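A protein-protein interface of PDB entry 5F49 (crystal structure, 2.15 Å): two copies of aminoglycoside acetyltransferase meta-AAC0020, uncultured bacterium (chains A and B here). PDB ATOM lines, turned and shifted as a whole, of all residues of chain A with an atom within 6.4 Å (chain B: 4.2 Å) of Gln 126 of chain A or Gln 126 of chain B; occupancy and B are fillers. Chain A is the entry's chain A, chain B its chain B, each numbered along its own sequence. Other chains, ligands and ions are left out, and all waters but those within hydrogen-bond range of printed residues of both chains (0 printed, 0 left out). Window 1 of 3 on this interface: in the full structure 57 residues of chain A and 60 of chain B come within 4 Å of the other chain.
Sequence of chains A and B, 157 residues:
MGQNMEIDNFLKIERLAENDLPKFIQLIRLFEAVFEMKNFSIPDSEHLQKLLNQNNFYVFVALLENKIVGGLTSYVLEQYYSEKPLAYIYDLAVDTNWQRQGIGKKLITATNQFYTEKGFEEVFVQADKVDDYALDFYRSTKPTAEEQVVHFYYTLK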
ATOM      1  N   TYR A  88      30.717 -13.124 -27.041  1.00  0.00           N
ATOM      2  CA  TYR A  88      30.101 -13.824 -25.922  1.00  0.00           C
ATOM      3  C   TYR A  88      30.207 -15.324 -26.133  1.00  0.00           C
ATOM      4  O   TYR A  88      29.487 -15.879 -26.956  1.00  0.00           O
ATOM      5  CB  TYR A  88      28.627 -13.412 -25.783  1.00  0.00           C
ATOM      6  CG  TYR A  88      27.859 -14.061 -24.645  1.00  0.00           C
ATOM      7  CD1 TYR A  88      28.514 -14.646 -23.568  1.00  0.00           C
ATOM      8  CD2 TYR A  88      26.472 -14.081 -24.651  1.00  0.00           C
ATOM      9  CE1 TYR A  88      27.811 -15.222 -22.534  1.00  0.00           C
ATOM     10  CE2 TYR A  88      25.760 -14.658 -23.622  1.00  0.00           C
ATOM     11  CZ  TYR A  88      26.431 -15.227 -22.569  1.00  0.00           C
ATOM     12  OH  TYR A  88      25.718 -15.800 -21.549  1.00  0.00           O
ATOM     13  N   ILE A  89      31.103 -15.976 -25.397  1.00  0.00           N
ATOM     14  CA  ILE A  89      31.174 -17.432 -25.421  1.00  0.00           C
ATOM     15  C   ILE A  89      29.969 -17.973 -24.674  1.00  0.00           C
ATOM     16  O   ILE A  89      29.804 -17.711 -23.485  1.00  0.00           O
ATOM     17  CB  ILE A  89      32.475 -17.959 -24.794  1.00  0.00           C
ATOM     18  CG1 ILE A  89      33.687 -17.422 -25.560  1.00  0.00           C
ATOM     19  CG2 ILE A  89      32.480 -19.488 -24.772  1.00  0.00           C
ATOM     20  CD1 ILE A  89      35.027 -17.798 -24.947  1.00  0.00           C
ATOM     21  N   TYR A  90      29.110 -18.708 -25.373  1.00  0.00           N
ATOM     22  CA  TYR A  90      27.860 -19.151 -24.774  1.00  0.00           C
ATOM     23  C   TYR A  90      27.954 -20.570 -24.200  1.00  0.00           C
ATOM     24  O   TYR A  90      27.605 -20.791 -23.040  1.00  0.00           O
ATOM     25  CB  TYR A  90      26.712 -19.064 -25.785  1.00  0.00           C
ATOM     26  CG  TYR A  90      25.359 -19.234 -25.134  1.00  0.00           C
ATOM     27  CD1 TYR A  90      24.791 -18.208 -24.392  1.00  0.00           C
ATOM     28  CD2 TYR A  90      24.663 -20.428 -25.235  1.00  0.00           C
ATOM     29  CE1 TYR A  90      23.562 -18.366 -23.781  1.00  0.00           C
ATOM     30  CE2 TYR A  90      23.433 -20.594 -24.625  1.00  0.00           C
ATOM     31  CZ  TYR A  90      22.888 -19.563 -23.903  1.00  0.00           C
ATOM     32  OH  TYR A  90      21.664 -19.731 -23.297  1.00  0.00           O
ATOM     33  N   PHE A 124      33.992 -12.550 -23.320  1.00  0.00           N
ATOM     34  CA  PHE A 124      33.594 -12.949 -21.975  1.00  0.00           C
ATOM     35  C   PHE A 124      32.800 -14.249 -21.975  1.00  0.00           C
ATOM     36  O   PHE A 124      32.225 -14.646 -22.990  1.00  0.00           O
ATOM     37  CB  PHE A 124      32.802 -11.833 -21.281  1.00  0.00           C
ATOM     38  CG  PHE A 124      31.463 -11.539 -21.901  1.00  0.00           C
ATOM     39  CD1 PHE A 124      31.350 -10.632 -22.943  1.00  0.00           C
ATOM     40  CD2 PHE A 124      30.313 -12.148 -21.423  1.00  0.00           C
ATOM     41  CE1 PHE A 124      30.112 -10.351 -23.506  1.00  0.00           C
ATOM     42  CE2 PHE A 124      29.075 -11.869 -21.975  1.00  0.00           C
ATOM     43  CZ  PHE A 124      28.971 -10.973 -23.018  1.00  0.00           C
ATOM     44  N   VAL A 125      32.791 -14.910 -20.824  1.00  0.00           N
ATOM     45  CA  VAL A 125      32.140 -16.203 -20.674  1.00  0.00           C
ATOM     46  C   VAL A 125      31.641 -16.334 -19.239  1.00  0.00           C
ATOM     47  O   VAL A 125      32.158 -15.677 -18.328  1.00  0.00           O
ATOM     48  CB  VAL A 125      33.107 -17.362 -21.026  1.00  0.00           C
ATOM     49  CG1 VAL A 125      34.213 -17.477 -19.972  1.00  0.00           C
ATOM     50  CG2 VAL A 125      32.356 -18.678 -21.190  1.00  0.00           C
ATOM     51  N   GLN A 126      30.617 -17.153 -19.030  1.00  0.00           N
ATOM     52  CA  GLN A 126      30.022 -17.268 -17.703  1.00  0.00           C
ATOM     53  C   GLN A 126      29.876 -18.714 -17.256  1.00  0.00           C
ATOM     54  O   GLN A 126      29.509 -19.584 -18.043  1.00  0.00           O
ATOM     55  CB  GLN A 126      28.661 -16.576 -17.680  1.00  0.00           C
ATOM     56  CG  GLN A 126      28.674 -15.217 -18.344  1.00  0.00           C
ATOM     57  CD  GLN A 126      27.475 -14.379 -17.991  1.00  0.00           C
ATOM     58  OE1 GLN A 126      26.337 -14.848 -18.043  1.00  0.00           O
ATOM     59  NE2 GLN A 126      27.721 -13.126 -17.621  1.00  0.00           N
ATOM     60  N   ALA A 127      30.160 -18.957 -15.982  1.00  0.00           N
ATOM     61  CA  ALA A 127      29.989 -20.275 -15.389  1.00  0.00           C
ATOM     62  C   ALA A 127      29.144 -20.167 -14.133  1.00  0.00           C
ATOM     63  O   ALA A 127      29.228 -19.172 -13.415  1.00  0.00           O
ATOM     64  CB  ALA A 127      31.322 -20.889 -15.076  1.00  0.00           C
ATOM     65  N   ASP A 128      28.325 -21.184 -13.873  1.00  0.00           N
ATOM     66  CA  ASP A 128      27.486 -21.193 -12.681  1.00  0.00           C
ATOM     67  C   ASP A 128      28.363 -21.280 -11.442  1.00  0.00           C
ATOM     68  O   ASP A 128      29.407 -21.938 -11.449  1.00  0.00           O
ATOM     69  CB  ASP A 128      26.490 -22.356 -12.712  1.00  0.00           C
ATOM     70  CG  ASP A 128      25.631 -22.354 -13.960  1.00  0.00           C
ATOM     71  OD1 ASP A 128      24.840 -21.399 -14.136  1.00  0.00           O
ATOM     72  OD2 ASP A 128      25.745 -23.307 -14.762  1.00  0.00           O
ATOM     73  N   TYR A 138      38.089 -22.154 -16.190  1.00  0.00           N
ATOM     74  CA  TYR A 138      38.200 -20.781 -16.680  1.00  0.00           C
ATOM     75  C   TYR A 138      39.289 -20.022 -15.931  1.00  0.00           C
ATOM     76  O   TYR A 138      40.028 -19.243 -16.524  1.00  0.00           O
ATOM     77  CB  TYR A 138      36.857 -20.043 -16.581  1.00  0.00           C
ATOM     78  CG  TYR A 138      35.860 -20.519 -17.615  1.00  0.00           C
ATOM     79  CD1 TYR A 138      36.115 -20.363 -18.970  1.00  0.00           C
ATOM     80  CD2 TYR A 138      34.679 -21.141 -17.239  1.00  0.00           C
ATOM     81  CE1 TYR A 138      35.224 -20.806 -19.918  1.00  0.00           C
ATOM     82  CE2 TYR A 138      33.772 -21.587 -18.189  1.00  0.00           C
ATOM     83  CZ  TYR A 138      34.052 -21.417 -19.524  1.00  0.00           C
ATOM     84  OH  TYR A 138      33.155 -21.854 -20.474  1.00  0.00           O
ATOM     85  N   VAL A 149      28.347 -12.283 -10.402  1.00  0.00           N
ATOM     86  CA  VAL A 149      27.200 -11.735 -11.107  1.00  0.00           C
ATOM     87  C   VAL A 149      25.929 -12.497 -10.726  1.00  0.00           C
ATOM     88  O   VAL A 149      25.981 -13.695 -10.438  1.00  0.00           O
ATOM     89  CB  VAL A 149      27.442 -11.776 -12.642  1.00  0.00           C
ATOM     90  CG1 VAL A 149      26.163 -11.550 -13.423  1.00  0.00           C
ATOM     91  CG2 VAL A 149      28.494 -10.742 -13.030  1.00  0.00           C
ATOM     92  N   VAL A 150      24.802 -11.791 -10.667  1.00  0.00           N
ATOM     93  CA  VAL A 150      23.509 -12.442 -10.498  1.00  0.00           C
ATOM     94  C   VAL A 150      22.733 -12.373 -11.814  1.00  0.00           C
ATOM     95  O   VAL A 150      22.615 -11.315 -12.443  1.00  0.00           O
ATOM     96  CB  VAL A 150      22.691 -11.820  -9.365  1.00  0.00           C
ATOM     97  CG1 VAL A 150      21.353 -12.531  -9.237  1.00  0.00           C
ATOM     98  CG2 VAL A 150      23.473 -11.884  -8.045  1.00  0.00           C
ATOM     99  N   HIS A 151      22.229 -13.524 -12.227  1.00  0.00           N
ATOM    100  CA  HIS A 151      21.591 -13.688 -13.520  1.00  0.00           C
ATOM    101  C   HIS A 151      20.096 -13.920 -13.326  1.00  0.00           C
ATOM    102  O   HIS A 151      19.697 -14.865 -12.658  1.00  0.00           O
ATOM    103  CB  HIS A 151      22.263 -14.854 -14.255  1.00  0.00           C
ATOM    104  CG  HIS A 151      21.584 -15.270 -15.521  1.00  0.00           C
ATOM    105  ND1 HIS A 151      22.016 -14.857 -16.767  1.00  0.00           N
ATOM    106  CD2 HIS A 151      20.542 -16.100 -15.742  1.00  0.00           C
ATOM    107  CE1 HIS A 151      21.253 -15.402 -17.694  1.00  0.00           C
ATOM    108  NE2 HIS A 151      20.346 -16.159 -17.102  1.00  0.00           N
ATOM    109  N   PHE A 152      19.276 -13.030 -13.877  1.00  0.00           N
ATOM    110  CA  PHE A 152      17.822 -13.133 -13.758  1.00  0.00           C
ATOM    111  C   PHE A 152      17.232 -13.544 -15.093  1.00  0.00           C
ATOM    112  O   PHE A 152      17.683 -13.072 -16.132  1.00  0.00           O
ATOM    113  CB  PHE A 152      17.199 -11.799 -13.329  1.00  0.00           C
ATOM    114  CG  PHE A 152      17.743 -11.244 -12.043  1.00  0.00           C
ATOM    115  CD1 PHE A 152      18.853 -10.404 -12.047  1.00  0.00           C
ATOM    116  CD2 PHE A 152      17.136 -11.542 -10.829  1.00  0.00           C
ATOM    117  CE1 PHE A 152      19.357  -9.886 -10.851  1.00  0.00           C
ATOM    118  CE2 PHE A 152      17.630 -11.027  -9.643  1.00  0.00           C
ATOM    119  CZ  PHE A 152      18.739 -10.193  -9.654  1.00  0.00           C
ATOM    120  N   TYR B  88      18.718 -10.943 -24.699  1.00  0.00           N
ATOM    121  CA  TYR B  88      19.699 -10.572 -23.681  1.00  0.00           C
ATOM    122  C   TYR B  88      19.642  -9.069 -23.433  1.00  0.00           C
ATOM    123  O   TYR B  88      20.068  -8.285 -24.278  1.00  0.00           O
ATOM    124  CB  TYR B  88      21.108 -10.991 -24.127  1.00  0.00           C
ATOM    125  CG  TYR B  88      22.259 -10.613 -23.205  1.00  0.00           C
ATOM    126  CD1 TYR B  88      22.051 -10.252 -21.875  1.00  0.00           C
ATOM    127  CD2 TYR B  88      23.566 -10.628 -23.673  1.00  0.00           C
ATOM    128  CE1 TYR B  88      23.114  -9.923 -21.045  1.00  0.00           C
ATOM    129  CE2 TYR B  88      24.627 -10.303 -22.852  1.00  0.00           C
ATOM    130  CZ  TYR B  88      24.394  -9.949 -21.543  1.00  0.00           C
ATOM    131  OH  TYR B  88      25.453  -9.622 -20.734  1.00  0.00           O
ATOM    132  N   VAL B 125      18.775 -10.997 -17.935  1.00  0.00           N
ATOM    133  CA  VAL B 125      19.482  -9.764 -17.610  1.00  0.00           C
ATOM    134  C   VAL B 125      20.396 -10.039 -16.418  1.00  0.00           C
ATOM    135  O   VAL B 125      20.113 -10.909 -15.584  1.00  0.00           O
ATOM    136  CB  VAL B 125      18.494  -8.605 -17.288  1.00  0.00           C
ATOM    137  CG1 VAL B 125      17.705  -8.905 -16.022  1.00  0.00           C
ATOM    138  CG2 VAL B 125      19.215  -7.269 -17.161  1.00  0.00           C
ATOM    139  N   GLN B 126      21.504  -9.316 -16.334  1.00  0.00           N
ATOM    140  CA  GLN B 126      22.442  -9.546 -15.248  1.00  0.00           C
ATOM    141  C   GLN B 126      22.747  -8.282 -14.467  1.00  0.00           C
ATOM    142  O   GLN B 126      22.622  -7.170 -14.985  1.00  0.00           O
ATOM    143  CB  GLN B 126      23.731 -10.149 -15.798  1.00  0.00           C
ATOM    144  CG  GLN B 126      23.495 -11.406 -16.611  1.00  0.00           C
ATOM    145  CD  GLN B 126      24.758 -12.201 -16.842  1.00  0.00           C
ATOM    146  OE1 GLN B 126      25.818 -11.640 -17.117  1.00  0.00           O
ATOM    147  NE2 GLN B 126      24.654 -13.521 -16.723  1.00  0.00           N
ATOM    148  N   ALA B 127      23.133  -8.474 -13.207  1.00  0.00           N
ATOM    149  CA  ALA B 127      23.601  -7.399 -12.346  1.00  0.00           C
ATOM    150  C   ALA B 127      24.792  -7.892 -11.525  1.00  0.00           C
ATOM    151  O   ALA B 127      24.889  -9.076 -11.193  1.00  0.00           O
ATOM    152  CB  ALA B 127      22.488  -6.917 -11.439  1.00  0.00           C
ATOM    153  N   VAL B 149      26.195 -16.523 -10.658  1.00  0.00           N
ATOM    154  CA  VAL B 149      27.173 -16.901 -11.675  1.00  0.00           C
ATOM    155  C   VAL B 149      28.456 -16.085 -11.581  1.00  0.00           C
ATOM    156  O   VAL B 149      28.500 -15.025 -10.953  1.00  0.00           O
ATOM    157  CB  VAL B 149      26.609 -16.740 -13.108  1.00  0.00           C
ATOM    158  CG1 VAL B 149      25.312 -17.531 -13.293  1.00  0.00           C
ATOM    159  CG2 VAL B 149      26.389 -15.277 -13.425  1.00  0.00           C
ATOM    160  N   VAL B 150      29.499 -16.595 -12.224  1.00  0.00           N
ATOM    161  CA  VAL B 150      30.794 -15.940 -12.259  1.00  0.00           C
ATOM    162  C   VAL B 150      31.110 -15.551 -13.691  1.00  0.00           C
ATOM    163  O   VAL B 150      31.101 -16.391 -14.602  1.00  0.00           O
ATOM    164  CB  VAL B 150      31.911 -16.843 -11.716  1.00  0.00           C
ATOM    165  CG1 VAL B 150      33.269 -16.170 -11.882  1.00  0.00           C
ATOM    166  CG2 VAL B 150      31.647 -17.210 -10.259  1.00  0.00           C
ATOM    167  N   HIS B 151      31.392 -14.270 -13.878  1.00  0.00           N
ATOM    168  CA  HIS B 151      31.633 -13.702 -15.194  1.00  0.00           C
ATOM    169  C   HIS B 151      33.137 -13.533 -15.446  1.00  0.00           C
ATOM    170  O   HIS B 151      33.805 -12.776 -14.742  1.00  0.00           O
ATOM    171  CB  HIS B 151      30.886 -12.368 -15.290  1.00  0.00           C
ATOM    172  CG  HIS B 151      31.167 -11.580 -16.532  1.00  0.00           C
ATOM    173  ND1 HIS B 151      30.342 -11.616 -17.637  1.00  0.00           N
ATOM    174  CD2 HIS B 151      32.152 -10.701 -16.825  1.00  0.00           C
ATOM    175  CE1 HIS B 151      30.822 -10.806 -18.566  1.00  0.00           C
ATOM    176  NE2 HIS B 151      31.919 -10.239 -18.099  1.00  0.00           N
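Phe 124 of chain A touches His 151 of chain B. O of Val 150 of chain B touches O of Val 125 of chain A (3.9 Å). Val 125 of chain A touches His 151 of chain B. O of Val 150 of chain B touches CA of Gln 126 of chain A, at 3.4 Å. CA of Val 149 of chain B touches O of Ala 127 of chain A, at 3.5 Å. Val 149 of chain B touches Asp 128 of chain A (CG1 to OD1, 3.99 Å). Val 149 of chain A touches Gln 126 of chain B (CG1 to CB, 3.7 Å). CG2 of Val 149 of chain A touches CB of His 151 of chain B (3.7 Å). Gln 126 of chain B touches Val 150 of chain A (CA to O, 3.3 Å). His 151 of chain A touches Val 125 of chain B.
Gln 126 of chain A touches just these residues of chain B: Gln 126, Val 150 and His 151. Of chain A, only Gln 126, Val 149, Val 150 and His 151 come within 4 Å of Gln 126 of chain B. Of the printed residues of chain B, Phe 152 of chain A touches Val 125 (2.8 Å). Printed residues of chain B within 4 Å of Ala 127 of chain A: Val 149 (3.5 Å) and Val 150 (2.9 Å). The nearest printed residue of chain B that does not touch Gln 126 of chain A is Val 149 of chain B (4.6 Å). The nearest printed residue of chain A that does not touch Val 150 of chain B is Val 149 of chain A (4.8 Å).
Gln 126 of chain A touches His 151 of chain B, and with the chains exchanged His 151 of chain A touches Gln 126 of chain B. Ala 127 of chain A touches Val 150 of chain B, and with the chains exchanged Val 150 of chain A touches Ala 127 of chain B. Val 149 of chain B touches its own counterpart, Val 149 of chain A. Val 149 of chain A touches His 151 of chain B, but with the chains exchanged His 151 of chain A does not touch Val 149 of chain B (4.2 Å). Positions printed for both chains: 88, 125, 126, 127, 149, 150 and 151. Of the 18 pairs that touch across the chains among the printed residues, 12 have their exchanged pair printed and touching as well.
The backbone NH (N) of Val 150 of chain A sits at hydrogen-bond distance from the backbone carbonyl oxygen (O) of Ala 127 of chain B (2.8 Å). OE1 of Gln 126 of chain B lies within hydrogen-bond range of NE2 of Gln 126 of chain A (2.5 Å). The backbone carbonyl oxygen (O) of Val 125 of chain B is in hydrogen-bond range of the backbone NH (N) of Phe 152 of chain A (2.8 Å). NE2 of Gln 126 of chain A sits at hydrogen-bond distance from ND1 of His 151 of chain B, 3.0 Å away. N of Val 149 of chain A sits at hydrogen-bond distance from O of Val 149 of chain B, 2.8 Å away. ND1 of His 151 of chain A is in hydrogen-bond range of NE2 of Gln 126 of chain B (3.0 Å). O of Ala 127 of chain A lies within hydrogen-bond range of N of Val 150 of chain B (2.9 Å).
The backbone carbonyl oxygen (O) of Phe 124 of chain A sits at hydrogen-bond distance from the backbone NH (N) of Ile 89 of chain A (3.0 Å).
Of the 7 printed residues of chain B, 6 touch a printed residue of chain A. Printed residues of chain B that touch a printed residue of chain A: Val 125, Gln 126, Ala 127, Val 149, Val 150 and His 151. Hydrophobic or aromatic side chains of chain B within 4 Å of the printed part of chain A: Val 125, Val 149, Val 150 and His 151. Of the 13 printed residues of chain A, 9 touch a printed residue of chain B. Hydrophobic or aromatic side chains of chain A within 4 Å of the printed part of chain B: Phe 124, Val 149, Val 150, His 151 and Phe 152.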
